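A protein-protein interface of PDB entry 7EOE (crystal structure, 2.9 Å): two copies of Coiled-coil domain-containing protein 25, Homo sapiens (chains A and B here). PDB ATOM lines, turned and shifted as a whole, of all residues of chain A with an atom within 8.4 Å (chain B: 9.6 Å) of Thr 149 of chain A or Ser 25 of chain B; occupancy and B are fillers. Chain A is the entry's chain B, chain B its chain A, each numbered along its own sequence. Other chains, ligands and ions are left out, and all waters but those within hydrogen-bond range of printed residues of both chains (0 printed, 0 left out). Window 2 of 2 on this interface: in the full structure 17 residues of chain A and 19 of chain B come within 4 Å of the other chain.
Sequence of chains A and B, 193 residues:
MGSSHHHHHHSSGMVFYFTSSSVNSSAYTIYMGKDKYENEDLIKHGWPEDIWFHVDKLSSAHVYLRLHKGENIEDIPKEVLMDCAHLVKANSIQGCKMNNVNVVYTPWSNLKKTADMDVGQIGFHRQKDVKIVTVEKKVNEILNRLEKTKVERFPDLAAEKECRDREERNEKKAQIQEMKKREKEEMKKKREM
Of the 14 printed residues of chain B, 4 touch a printed residue of chain A. Hydrophobic or aromatic side chains of chain A within 4 Å of the printed part of chain B: Ala 27. Among the printed residues, 4 pairs touch across the chains. Among the printed residues, no Asp or Glu carboxylate lies within 4 Å of a Lys or Arg side-chain nitrogen of the other chain.
Ala 27 of chain B touches Ala 27 of chain A (CB to CB, 3.5 Å). NZ of Lys 148 of chain A touches O of Val 23 of chain B (3.996 Å). Lys 148 of chain A touches Asn 24 of chain B (CE to O, 3.0 Å). O of Ser 25 of chain B touches CG2 of Thr 149 of chain A, at 3.2 Å.
The side-chain hydroxyl of Ser 22 of chain B sits at hydrogen-bond distance from the side-chain amide oxygen of Asn 24 of chain B, at 2.6 Å. The side-chain carboxylate (OE2) of Glu 79 of chain B lies within hydrogen-bond range of the backbone NH (N) of Val 23 of chain B, at 2.5 Å. The side-chain amide oxygen (OD1) of Asn 24 of chain B lies within hydrogen-bond range of the backbone NH (N) of Ser 26 of chain B (2.5 Å). The backbone carbonyl oxygen (O) of Ala 27 of chain B sits at hydrogen-bond distance from a ring nitrogen (NE2) of His 68 of chain B, at 3.4 Å. N of Thr 19 of chain A is in hydrogen-bond range of OG1 of Thr 149 of chain A, at 2.9 Å. O of Leu 146 of chain A lies within hydrogen-bond range of OG1 of Thr 149 of chain A, at 2.7 Å.
Ala 27 of chain B touches its own counterpart, Ala 27 of chain A. Of the 4 pairs that touch across the chains among the printed residues, 1 has its exchanged pair printed and touching as well.
Thr 149 of chain A touches one residue of chain B. Ser 25 of chain B touches one residue of chain A. Thr 19 of chain A touches none of the printed residues of chain B. No residue of chain A comes within 4 Å of Ser 26 of chain B. Printed residues of chain A within 4 Å of Asn 24 of chain B: Lys 148. Of the printed residues of chain A, Ala 27 of chain B touches Ala 27. Printed residues of chain B within 4 Å of Ala 27 of chain A: Ala 27. Printed residues of chain B within 4 Å of Lys 148 of chain A: Val 23 and Asn 24. Of the printed residues of chain A, Val 23 of chain B touches Lys 148 (3.996 Å). Glu 79 of chain B touches none of the printed residues of chain A. The nearest residue of chain B that does not touch Thr 149 of chain A is Ser 26 of chain B (4.5 Å). The nearest printed residue of chain B that does not touch Ala 27 of chain A is Thr 19 of chain B (4.2 Å).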
ATOM      1  N   PHE A  16       2.513  23.546 -31.261  1.00  0.00           N
ATOM      2  CA  PHE A  16       1.693  22.630 -30.482  1.00  0.00           C
ATOM      3  C   PHE A  16       0.940  23.396 -29.403  1.00  0.00           C
ATOM      4  O   PHE A  16       1.463  24.353 -28.824  1.00  0.00           O
ATOM      5  CB  PHE A  16       2.555  21.543 -29.837  1.00  0.00           C
ATOM      6  CG  PHE A  16       3.356  20.736 -30.818  1.00  0.00           C
ATOM      7  CD1 PHE A  16       2.740  19.823 -31.657  1.00  0.00           C
ATOM      8  CD2 PHE A  16       4.732  20.882 -30.891  1.00  0.00           C
ATOM      9  CE1 PHE A  16       3.478  19.077 -32.554  1.00  0.00           C
ATOM     10  CE2 PHE A  16       5.476  20.138 -31.788  1.00  0.00           C
ATOM     11  CZ  PHE A  16       4.848  19.234 -32.620  1.00  0.00           C
ATOM     12  N   TYR A  17      -0.285  22.955 -29.124  1.00  0.00           N
ATOM     13  CA  TYR A  17      -1.154  23.585 -28.137  1.00  0.00           C
ATOM     14  C   TYR A  17      -1.771  22.503 -27.264  1.00  0.00           C
ATOM     15  O   TYR A  17      -2.462  21.612 -27.768  1.00  0.00           O
ATOM     16  CB  TYR A  17      -2.248  24.418 -28.814  1.00  0.00           C
ATOM     17  CG  TYR A  17      -1.742  25.643 -29.544  1.00  0.00           C
ATOM     18  CD1 TYR A  17      -1.749  26.890 -28.934  1.00  0.00           C
ATOM     19  CD2 TYR A  17      -1.265  25.555 -30.846  1.00  0.00           C
ATOM     20  CE1 TYR A  17      -1.292  28.015 -29.596  1.00  0.00           C
ATOM     21  CE2 TYR A  17      -0.805  26.675 -31.518  1.00  0.00           C
ATOM     22  CZ  TYR A  17      -0.820  27.902 -30.886  1.00  0.00           C
ATOM     23  OH  TYR A  17      -0.364  29.021 -31.545  1.00  0.00           O
ATOM     24  N   PHE A  18      -1.523  22.588 -25.961  1.00  0.00           N
ATOM     25  CA  PHE A  18      -2.066  21.689 -24.959  1.00  0.00           C
ATOM     26  C   PHE A  18      -2.987  22.464 -24.025  1.00  0.00           C
ATOM     27  O   PHE A  18      -2.920  23.694 -23.929  1.00  0.00           O
ATOM     28  CB  PHE A  18      -0.948  21.023 -24.145  1.00  0.00           C
ATOM     29  CG  PHE A  18       0.246  20.615 -24.962  1.00  0.00           C
ATOM     30  CD1 PHE A  18       0.347  19.334 -25.475  1.00  0.00           C
ATOM     31  CD2 PHE A  18       1.274  21.512 -25.209  1.00  0.00           C
ATOM     32  CE1 PHE A  18       1.449  18.957 -26.218  1.00  0.00           C
ATOM     33  CE2 PHE A  18       2.374  21.142 -25.956  1.00  0.00           C
ATOM     34  CZ  PHE A  18       2.461  19.862 -26.463  1.00  0.00           C
ATOM     35  N   THR A  19      -3.842  21.723 -23.322  1.00  0.00           N
ATOM     36  CA  THR A  19      -4.815  22.286 -22.392  1.00  0.00           C
ATOM     37  C   THR A  19      -4.510  21.783 -20.988  1.00  0.00           C
ATOM     38  O   THR A  19      -4.492  20.570 -20.752  1.00  0.00           O
ATOM     39  CB  THR A  19      -6.243  21.916 -22.796  1.00  0.00           C
ATOM     40  OG1 THR A  19      -6.561  22.534 -24.050  1.00  0.00           O
ATOM     41  CG2 THR A  19      -7.233  22.382 -21.740  1.00  0.00           C
ATOM     42  N   SER A  20      -4.268  22.711 -20.063  1.00  0.00           N
ATOM     43  CA  SER A  20      -4.045  22.398 -18.653  1.00  0.00           C
ATOM     44  C   SER A  20      -5.260  22.842 -17.843  1.00  0.00           C
ATOM     45  O   SER A  20      -5.526  24.042 -17.722  1.00  0.00           O
ATOM     46  CB  SER A  20      -2.772  23.067 -18.143  1.00  0.00           C
ATOM     47  OG  SER A  20      -2.450  22.617 -16.838  1.00  0.00           O
ATOM     48  N   SER A  21      -5.993  21.875 -17.293  1.00  0.00           N
ATOM     49  CA  SER A  21      -7.169  22.149 -16.475  1.00  0.00           C
ATOM     50  C   SER A  21      -6.771  22.308 -15.011  1.00  0.00           C
ATOM     51  O   SER A  21      -6.013  21.492 -14.475  1.00  0.00           O
ATOM     52  CB  SER A  21      -8.197  21.025 -16.626  1.00  0.00           C
ATOM     53  OG  SER A  21      -8.538  20.827 -17.986  1.00  0.00           O
ATOM     54  N   ALA A  27      -9.720  26.332 -18.256  1.00  0.00           N
ATOM     55  CA  ALA A  27      -8.686  25.739 -19.089  1.00  0.00           C
ATOM     56  C   ALA A  27      -7.615  26.769 -19.416  1.00  0.00           C
ATOM     57  O   ALA A  27      -7.923  27.868 -19.884  1.00  0.00           O
ATOM     58  CB  ALA A  27      -9.284  25.181 -20.377  1.00  0.00           C
ATOM     59  N   TYR A  28      -6.361  26.402 -19.176  1.00  0.00           N
ATOM     60  CA  TYR A  28      -5.220  27.231 -19.524  1.00  0.00           C
ATOM     61  C   TYR A  28      -4.570  26.698 -20.793  1.00  0.00           C
ATOM     62  O   TYR A  28      -4.386  25.487 -20.949  1.00  0.00           O
ATOM     63  CB  TYR A  28      -4.201  27.265 -18.383  1.00  0.00           C
ATOM     64  CG  TYR A  28      -4.665  28.049 -17.176  1.00  0.00           C
ATOM     65  CD1 TYR A  28      -4.206  29.339 -16.942  1.00  0.00           C
ATOM     66  CD2 TYR A  28      -5.572  27.503 -16.276  1.00  0.00           C
ATOM     67  CE1 TYR A  28      -4.631  30.059 -15.840  1.00  0.00           C
ATOM     68  CE2 TYR A  28      -6.003  28.215 -15.173  1.00  0.00           C
ATOM     69  CZ  TYR A  28      -5.529  29.492 -14.960  1.00  0.00           C
ATOM     70  OH  TYR A  28      -5.957  30.203 -13.862  1.00  0.00           O
ATOM     71  N   THR A  29      -4.228  27.609 -21.700  1.00  0.00           N
ATOM     72  CA  THR A  29      -3.617  27.243 -22.968  1.00  0.00           C
ATOM     73  C   THR A  29      -2.100  27.249 -22.838  1.00  0.00           C
ATOM     74  O   THR A  29      -1.511  28.229 -22.369  1.00  0.00           O
ATOM     75  CB  THR A  29      -4.052  28.199 -24.080  1.00  0.00           C
ATOM     76  OG1 THR A  29      -5.451  28.029 -24.340  1.00  0.00           O
ATOM     77  CG2 THR A  29      -3.267  27.929 -25.357  1.00  0.00           C
ATOM     78  N   ILE A  30      -1.476  26.149 -23.249  1.00  0.00           N
ATOM     79  CA  ILE A  30      -0.027  26.022 -23.310  1.00  0.00           C
ATOM     80  C   ILE A  30       0.351  25.822 -24.770  1.00  0.00           C
ATOM     81  O   ILE A  30      -0.356  25.128 -25.503  1.00  0.00           O
ATOM     82  CB  ILE A  30       0.470  24.848 -22.440  1.00  0.00           C
ATOM     83  CG1 ILE A  30       0.038  25.038 -20.985  1.00  0.00           C
ATOM     84  CG2 ILE A  30       1.977  24.703 -22.531  1.00  0.00           C
ATOM     85  CD1 ILE A  30       0.262  23.821 -20.118  1.00  0.00           C
ATOM     86  N   ASP A  83       2.230  21.472 -14.654  1.00  0.00           N
ATOM     87  CA  ASP A  83       2.007  20.987 -16.012  1.00  0.00           C
ATOM     88  C   ASP A  83       3.009  21.604 -16.975  1.00  0.00           C
ATOM     89  O   ASP A  83       3.608  20.906 -17.803  1.00  0.00           O
ATOM     90  CB  ASP A  83       0.580  21.301 -16.453  1.00  0.00           C
ATOM     91  CG  ASP A  83      -0.439  20.429 -15.766  1.00  0.00           C
ATOM     92  OD1 ASP A  83      -0.063  19.724 -14.807  1.00  0.00           O
ATOM     93  OD2 ASP A  83      -1.616  20.439 -16.184  1.00  0.00           O
ATOM     94  N   GLU A 141       1.342  10.854 -15.897  1.00  0.00           N
ATOM     95  CA  GLU A 141      -0.049  11.237 -16.116  1.00  0.00           C
ATOM     96  C   GLU A 141      -0.155  12.680 -16.592  1.00  0.00           C
ATOM     97  O   GLU A 141      -1.043  13.017 -17.382  1.00  0.00           O
ATOM     98  CB  GLU A 141      -0.862  11.016 -14.837  1.00  0.00           C
ATOM     99  CG  GLU A 141      -2.250  11.674 -14.820  1.00  0.00           C
ATOM    100  CD  GLU A 141      -2.248  13.142 -14.378  1.00  0.00           C
ATOM    101  OE1 GLU A 141      -1.165  13.647 -14.007  1.00  0.00           O
ATOM    102  OE2 GLU A 141      -3.334  13.772 -14.410  1.00  0.00           O
ATOM    103  N   ILE A 142       0.736  13.552 -16.114  1.00  0.00           N
ATOM    104  CA  ILE A 142       0.722  14.943 -16.560  1.00  0.00           C
ATOM    105  C   ILE A 142       0.965  15.018 -18.063  1.00  0.00           C
ATOM    106  O   ILE A 142       0.271  15.741 -18.787  1.00  0.00           O
ATOM    107  CB  ILE A 142       1.754  15.775 -15.778  1.00  0.00           C
ATOM    108  CG1 ILE A 142       1.209  16.146 -14.396  1.00  0.00           C
ATOM    109  CG2 ILE A 142       2.141  17.021 -16.555  1.00  0.00           C
ATOM    110  CD1 ILE A 142       2.138  17.042 -13.599  1.00  0.00           C
ATOM    111  N   LEU A 143       1.947  14.261 -18.556  1.00  0.00           N
ATOM    112  CA  LEU A 143       2.297  14.327 -19.970  1.00  0.00           C
ATOM    113  C   LEU A 143       1.281  13.597 -20.841  1.00  0.00           C
ATOM    114  O   LEU A 143       0.978  14.045 -21.953  1.00  0.00           O
ATOM    115  CB  LEU A 143       3.696  13.754 -20.184  1.00  0.00           C
ATOM    116  CG  LEU A 143       4.797  14.453 -19.386  1.00  0.00           C
ATOM    117  CD1 LEU A 143       6.032  13.575 -19.300  1.00  0.00           C
ATOM    118  CD2 LEU A 143       5.127  15.801 -19.999  1.00  0.00           C
ATOM    119  N   ASN A 144       0.746  12.474 -20.354  1.00  0.00           N
ATOM    120  CA  ASN A 144      -0.296  11.766 -21.091  1.00  0.00           C
ATOM    121  C   ASN A 144      -1.545  12.629 -21.212  1.00  0.00           C
ATOM    122  O   ASN A 144      -2.071  12.840 -22.312  1.00  0.00           O
ATOM    123  CB  ASN A 144      -0.624  10.450 -20.384  1.00  0.00           C
ATOM    124  CG  ASN A 144       0.541   9.478 -20.382  1.00  0.00           C
ATOM    125  OD1 ASN A 144       1.628   9.787 -20.870  1.00  0.00           O
ATOM    126  ND2 ASN A 144       0.321   8.297 -19.818  1.00  0.00           N
ATOM    127  N   ARG A 145      -2.029  13.137 -20.077  1.00  0.00           N
ATOM    128  CA  ARG A 145      -3.187  14.024 -20.067  1.00  0.00           C
ATOM    129  C   ARG A 145      -2.942  15.257 -20.926  1.00  0.00           C
ATOM    130  O   ARG A 145      -3.847  15.721 -21.629  1.00  0.00           O
ATOM    131  CB  ARG A 145      -3.518  14.427 -18.626  1.00  0.00           C
ATOM    132  CG  ARG A 145      -4.605  15.485 -18.488  1.00  0.00           C
ATOM    133  CD  ARG A 145      -4.833  15.864 -17.034  1.00  0.00           C
ATOM    134  NE  ARG A 145      -3.620  16.388 -16.424  1.00  0.00           N
ATOM    135  CZ  ARG A 145      -3.171  17.627 -16.583  1.00  0.00           C
ATOM    136  NH1 ARG A 145      -3.836  18.498 -17.332  1.00  0.00           N
ATOM    137  NH2 ARG A 145      -2.047  17.990 -15.986  1.00  0.00           N
ATOM    138  N   LEU A 146      -1.720  15.799 -20.885  1.00  0.00           N
ATOM    139  CA  LEU A 146      -1.427  17.012 -21.641  1.00  0.00           C
ATOM    140  C   LEU A 146      -1.387  16.750 -23.142  1.00  0.00           C
ATOM    141  O   LEU A 146      -1.807  17.601 -23.934  1.00  0.00           O
ATOM    142  CB  LEU A 146      -0.104  17.614 -21.169  1.00  0.00           C
ATOM    143  CG  LEU A 146      -0.174  18.633 -20.026  1.00  0.00           C
ATOM    144  CD1 LEU A 146       1.160  19.347 -19.858  1.00  0.00           C
ATOM    145  CD2 LEU A 146      -1.294  19.636 -20.250  1.00  0.00           C
ATOM    146  N   GLU A 147      -0.901  15.577 -23.558  1.00  0.00           N
ATOM    147  CA  GLU A 147      -0.822  15.289 -24.987  1.00  0.00           C
ATOM    148  C   GLU A 147      -2.158  14.835 -25.556  1.00  0.00           C
ATOM    149  O   GLU A 147      -2.434  15.070 -26.738  1.00  0.00           O
ATOM    150  CB  GLU A 147       0.254  14.237 -25.269  1.00  0.00           C
ATOM    151  CG  GLU A 147       0.324  13.840 -26.739  1.00  0.00           C
ATOM    152  CD  GLU A 147       1.733  13.687 -27.257  1.00  0.00           C
ATOM    153  OE1 GLU A 147       2.514  14.657 -27.155  1.00  0.00           O
ATOM    154  OE2 GLU A 147       2.054  12.601 -27.783  1.00  0.00           O
ATOM    155  N   LYS A 148      -3.004  14.202 -24.743  1.00  0.00           N
ATOM    156  CA  LYS A 148      -4.344  13.867 -25.208  1.00  0.00           C
ATOM    157  C   LYS A 148      -5.107  15.116 -25.645  1.00  0.00           C
ATOM    158  O   LYS A 148      -6.075  15.013 -26.407  1.00  0.00           O
ATOM    159  CB  LYS A 148      -5.089  13.106 -24.102  1.00  0.00           C
ATOM    160  CG  LYS A 148      -6.565  12.849 -24.351  1.00  0.00           C
ATOM    161  CD  LYS A 148      -7.142  11.889 -23.319  1.00  0.00           C
ATOM    162  CE  LYS A 148      -8.661  11.935 -23.308  1.00  0.00           C
ATOM    163  NZ  LYS A 148      -9.270  11.052 -22.275  1.00  0.00           N
ATOM    164  N   THR A 149      -4.667  16.296 -25.207  1.00  0.00           N
ATOM    165  CA  THR A 149      -5.238  17.564 -25.631  1.00  0.00           C
ATOM    166  C   THR A 149      -4.394  18.263 -26.693  1.00  0.00           C
ATOM    167  O   THR A 149      -4.614  19.449 -26.958  1.00  0.00           O
ATOM    168  CB  THR A 149      -5.417  18.480 -24.419  1.00  0.00           C
ATOM    169  OG1 THR A 149      -4.137  18.954 -23.985  1.00  0.00           O
ATOM    170  CG2 THR A 149      -6.069  17.721 -23.275  1.00  0.00           C
ATOM    171  N   LYS A 150      -3.435  17.565 -27.301  1.00  0.00           N
ATOM    172  CA  LYS A 150      -2.495  18.203 -28.217  1.00  0.00           C
ATOM    173  C   LYS A 150      -3.165  18.512 -29.552  1.00  0.00           C
ATOM    174  O   LYS A 150      -3.659  17.611 -30.239  1.00  0.00           O
ATOM    175  CB  LYS A 150      -1.259  17.330 -28.424  1.00  0.00           C
ATOM    176  CG  LYS A 150      -0.093  18.056 -29.082  1.00  0.00           C
ATOM    177  CD  LYS A 150       1.142  17.174 -29.140  1.00  0.00           C
ATOM    178  CE  LYS A 150       1.263  16.469 -30.470  1.00  0.00           C
ATOM    179  NZ  LYS A 150       2.299  15.406 -30.412  1.00  0.00           N
ATOM    180  N   VAL A 151      -3.189  19.794 -29.901  1.00  0.00           N
ATOM    181  CA  VAL A 151      -3.661  20.287 -31.188  1.00  0.00           C
ATOM    182  C   VAL A 151      -2.478  20.941 -31.886  1.00  0.00           C
ATOM    183  O   VAL A 151      -1.706  21.668 -31.254  1.00  0.00           O
ATOM    184  CB  VAL A 151      -4.832  21.280 -31.036  1.00  0.00           C
ATOM    185  CG1 VAL A 151      -5.459  21.573 -32.389  1.00  0.00           C
ATOM    186  CG2 VAL A 151      -5.872  20.728 -30.078  1.00  0.00           C
ATOM    187  N   GLU A 152      -2.327  20.685 -33.182  1.00  0.00           N
ATOM    188  CA  GLU A 152      -1.248  21.274 -33.963  1.00  0.00           C
ATOM    189  C   GLU A 152      -1.812  22.341 -34.886  1.00  0.00           C
ATOM    190  O   GLU A 152      -2.759  22.082 -35.636  1.00  0.00           O
ATOM    191  CB  GLU A 152      -0.532  20.208 -34.794  1.00  0.00           C
ATOM    192  CG  GLU A 152      -0.275  18.911 -34.060  1.00  0.00           C
ATOM    193  CD  GLU A 152      -0.260  17.726 -34.997  1.00  0.00           C
ATOM    194  OE1 GLU A 152      -0.714  17.881 -36.150  1.00  0.00           O
ATOM    195  OE2 GLU A 152       0.205  16.644 -34.582  1.00  0.00           O
ATOM    196  N   THR B  19     -16.341  28.016 -20.906  1.00  0.00           N
ATOM    197  CA  THR B  19     -15.526  26.838 -21.169  1.00  0.00           C
ATOM    198  C   THR B  19     -16.290  25.609 -20.704  1.00  0.00           C
ATOM    199  O   THR B  19     -16.627  25.497 -19.520  1.00  0.00           O
ATOM    200  CB  THR B  19     -14.174  26.928 -20.457  1.00  0.00           C
ATOM    201  OG1 THR B  19     -13.408  28.002 -21.014  1.00  0.00           O
ATOM    202  CG2 THR B  19     -13.406  25.625 -20.609  1.00  0.00           C
ATOM    203  N   SER B  20     -16.571  24.700 -21.632  1.00  0.00           N
ATOM    204  CA  SER B  20     -17.197  23.423 -21.308  1.00  0.00           C
ATOM    205  C   SER B  20     -16.155  22.327 -21.485  1.00  0.00           C
ATOM    206  O   SER B  20     -15.796  21.980 -22.614  1.00  0.00           O
ATOM    207  CB  SER B  20     -18.418  23.172 -22.191  1.00  0.00           C
ATOM    208  OG  SER B  20     -19.133  22.026 -21.759  1.00  0.00           O
ATOM    209  N   SER B  21     -15.685  21.773 -20.372  1.00  0.00           N
ATOM    210  CA  SER B  21     -14.726  20.681 -20.402  1.00  0.00           C
ATOM    211  C   SER B  21     -15.483  19.363 -20.405  1.00  0.00           C
ATOM    212  O   SER B  21     -16.400  19.165 -19.601  1.00  0.00           O
ATOM    213  CB  SER B  21     -13.782  20.746 -19.203  1.00  0.00           C
ATOM    214  OG  SER B  21     -14.438  20.317 -18.025  1.00  0.00           O
ATOM    215  N   SER B  22     -15.114  18.475 -21.311  1.00  0.00           N
ATOM    216  CA  SER B  22     -15.760  17.182 -21.404  1.00  0.00           C
ATOM    217  C   SER B  22     -14.907  16.108 -20.725  1.00  0.00           C
ATOM    218  O   SER B  22     -13.921  16.399 -20.039  1.00  0.00           O
ATOM    219  CB  SER B  22     -16.064  16.880 -22.871  1.00  0.00           C
ATOM    220  OG  SER B  22     -14.890  16.569 -23.581  1.00  0.00           O
ATOM    221  N   VAL B  23     -15.289  14.842 -20.917  1.00  0.00           N
ATOM    222  CA  VAL B  23     -14.561  13.745 -20.288  1.00  0.00           C
ATOM    223  C   VAL B  23     -13.265  13.427 -21.019  1.00  0.00           C
ATOM    224  O   VAL B  23     -12.396  12.749 -20.454  1.00  0.00           O
ATOM    225  CB  VAL B  23     -15.430  12.481 -20.197  1.00  0.00           C
ATOM    226  CG1 VAL B  23     -16.473  12.633 -19.096  1.00  0.00           C
ATOM    227  CG2 VAL B  23     -16.073  12.164 -21.545  1.00  0.00           C
ATOM    228  N   ASN B  24     -13.114  13.888 -22.260  1.00  0.00           N
ATOM    229  CA  ASN B  24     -11.863  13.778 -23.000  1.00  0.00           C
ATOM    230  C   ASN B  24     -10.777  14.695 -22.466  1.00  0.00           C
ATOM    231  O   ASN B  24      -9.691  14.756 -23.053  1.00  0.00           O
ATOM    232  CB  ASN B  24     -12.099  14.093 -24.480  1.00  0.00           C
ATOM    233  CG  ASN B  24     -12.592  15.512 -24.706  1.00  0.00           C
ATOM    234  OD1 ASN B  24     -12.342  16.425 -23.916  1.00  0.00           O
ATOM    235  ND2 ASN B  24     -13.334  15.695 -25.784  1.00  0.00           N
ATOM    236  N   SER B  25     -11.073  15.455 -21.418  1.00  0.00           N
ATOM    237  CA  SER B  25     -10.175  16.453 -20.860  1.00  0.00           C
ATOM    238  C   SER B  25      -9.787  17.541 -21.860  1.00  0.00           C
ATOM    239  O   SER B  25      -8.752  18.180 -21.684  1.00  0.00           O
ATOM    240  CB  SER B  25      -8.906  15.801 -20.286  1.00  0.00           C
ATOM    241  OG  SER B  25      -9.165  15.149 -19.051  1.00  0.00           O
ATOM    242  N   SER B  26     -10.585  17.799 -22.902  1.00  0.00           N
ATOM    243  CA  SER B  26     -10.345  18.937 -23.788  1.00  0.00           C
ATOM    244  C   SER B  26     -11.435  19.974 -23.559  1.00  0.00           C
ATOM    245  O   SER B  26     -12.606  19.628 -23.378  1.00  0.00           O
ATOM    246  CB  SER B  26     -10.321  18.579 -25.282  1.00  0.00           C
ATOM    247  OG  SER B  26     -11.528  17.991 -25.717  1.00  0.00           O
ATOM    248  N   ALA B  27     -11.046  21.243 -23.556  1.00  0.00           N
ATOM    249  CA  ALA B  27     -11.982  22.332 -23.321  1.00  0.00           C
ATOM    250  C   ALA B  27     -12.617  22.791 -24.627  1.00  0.00           C
ATOM    251  O   ALA B  27     -11.918  23.031 -25.617  1.00  0.00           O
ATOM    252  CB  ALA B  27     -11.277  23.508 -22.650  1.00  0.00           C
ATOM    253  N   TYR B  28     -13.942  22.897 -24.623  1.00  0.00           N
ATOM    254  CA  TYR B  28     -14.699  23.442 -25.738  1.00  0.00           C
ATOM    255  C   TYR B  28     -15.080  24.883 -25.428  1.00  0.00           C
ATOM    256  O   TYR B  28     -15.526  25.194 -24.317  1.00  0.00           O
ATOM    257  CB  TYR B  28     -15.959  22.618 -26.009  1.00  0.00           C
ATOM    258  CG  TYR B  28     -15.704  21.269 -26.641  1.00  0.00           C
ATOM    259  CD1 TYR B  28     -15.946  21.063 -27.992  1.00  0.00           C
ATOM    260  CD2 TYR B  28     -15.233  20.202 -25.890  1.00  0.00           C
ATOM    261  CE1 TYR B  28     -15.721  19.835 -28.577  1.00  0.00           C
ATOM    262  CE2 TYR B  28     -15.002  18.969 -26.467  1.00  0.00           C
ATOM    263  CZ  TYR B  28     -15.247  18.791 -27.812  1.00  0.00           C
ATOM    264  OH  TYR B  28     -15.020  17.565 -28.393  1.00  0.00           O
ATOM    265  N   HIS B  68     -13.044  21.756 -32.473  1.00  0.00           N
ATOM    266  CA  HIS B  68     -11.625  21.653 -32.760  1.00  0.00           C
ATOM    267  C   HIS B  68     -11.408  21.342 -34.238  1.00  0.00           C
ATOM    268  O   HIS B  68     -12.345  21.050 -34.986  1.00  0.00           O
ATOM    269  CB  HIS B  68     -10.974  20.573 -31.895  1.00  0.00           C
ATOM    270  CG  HIS B  68     -11.230  20.731 -30.430  1.00  0.00           C
ATOM    271  ND1 HIS B  68     -12.433  20.400 -29.844  1.00  0.00           N
ATOM    272  CD2 HIS B  68     -10.437  21.184 -29.430  1.00  0.00           C
ATOM    273  CE1 HIS B  68     -12.371  20.641 -28.547  1.00  0.00           C
ATOM    274  NE2 HIS B  68     -11.171  21.117 -28.270  1.00  0.00           N
ATOM    275  N   PRO B  77     -19.416  15.702 -27.849  1.00  0.00           N
ATOM    276  CA  PRO B  77     -19.739  14.972 -26.618  1.00  0.00           C
ATOM    277  C   PRO B  77     -21.069  15.431 -26.038  1.00  0.00           C
ATOM    278  O   PRO B  77     -21.462  16.593 -26.170  1.00  0.00           O
ATOM    279  CB  PRO B  77     -18.572  15.313 -25.685  1.00  0.00           C
ATOM    280  CG  PRO B  77     -17.448  15.660 -26.601  1.00  0.00           C
ATOM    281  CD  PRO B  77     -18.074  16.307 -27.803  1.00  0.00           C
ATOM    282  N   GLU B  79     -22.039  15.801 -22.920  1.00  0.00           N
ATOM    283  CA  GLU B  79     -21.925  16.809 -21.871  1.00  0.00           C
ATOM    284  C   GLU B  79     -21.816  18.210 -22.460  1.00  0.00           C
ATOM    285  O   GLU B  79     -22.447  19.150 -21.964  1.00  0.00           O
ATOM    286  CB  GLU B  79     -20.728  16.509 -20.969  1.00  0.00           C
ATOM    287  CG  GLU B  79     -19.404  16.376 -21.694  1.00  0.00           C
ATOM    288  CD  GLU B  79     -18.885  14.959 -21.702  1.00  0.00           C
ATOM    289  OE1 GLU B  79     -19.636  14.049 -22.109  1.00  0.00           O
ATOM    290  OE2 GLU B  79     -17.730  14.752 -21.285  1.00  0.00           O
ATOM    291  N   VAL B  80     -21.017  18.370 -23.517  1.00  0.00           N
ATOM    292  CA  VAL B  80     -20.862  19.679 -24.142  1.00  0.00           C
ATOM    293  C   VAL B  80     -22.156  20.103 -24.824  1.00  0.00           C
ATOM    294  O   VAL B  80     -22.581  21.263 -24.719  1.00  0.00           O
ATOM    295  CB  VAL B  80     -19.682  19.653 -25.130  1.00  0.00           C
ATOM    296  CG1 VAL B  80     -19.533  20.999 -25.821  1.00  0.00           C
ATOM    297  CG2 VAL B  80     -18.398  19.267 -24.412  1.00  0.00           C
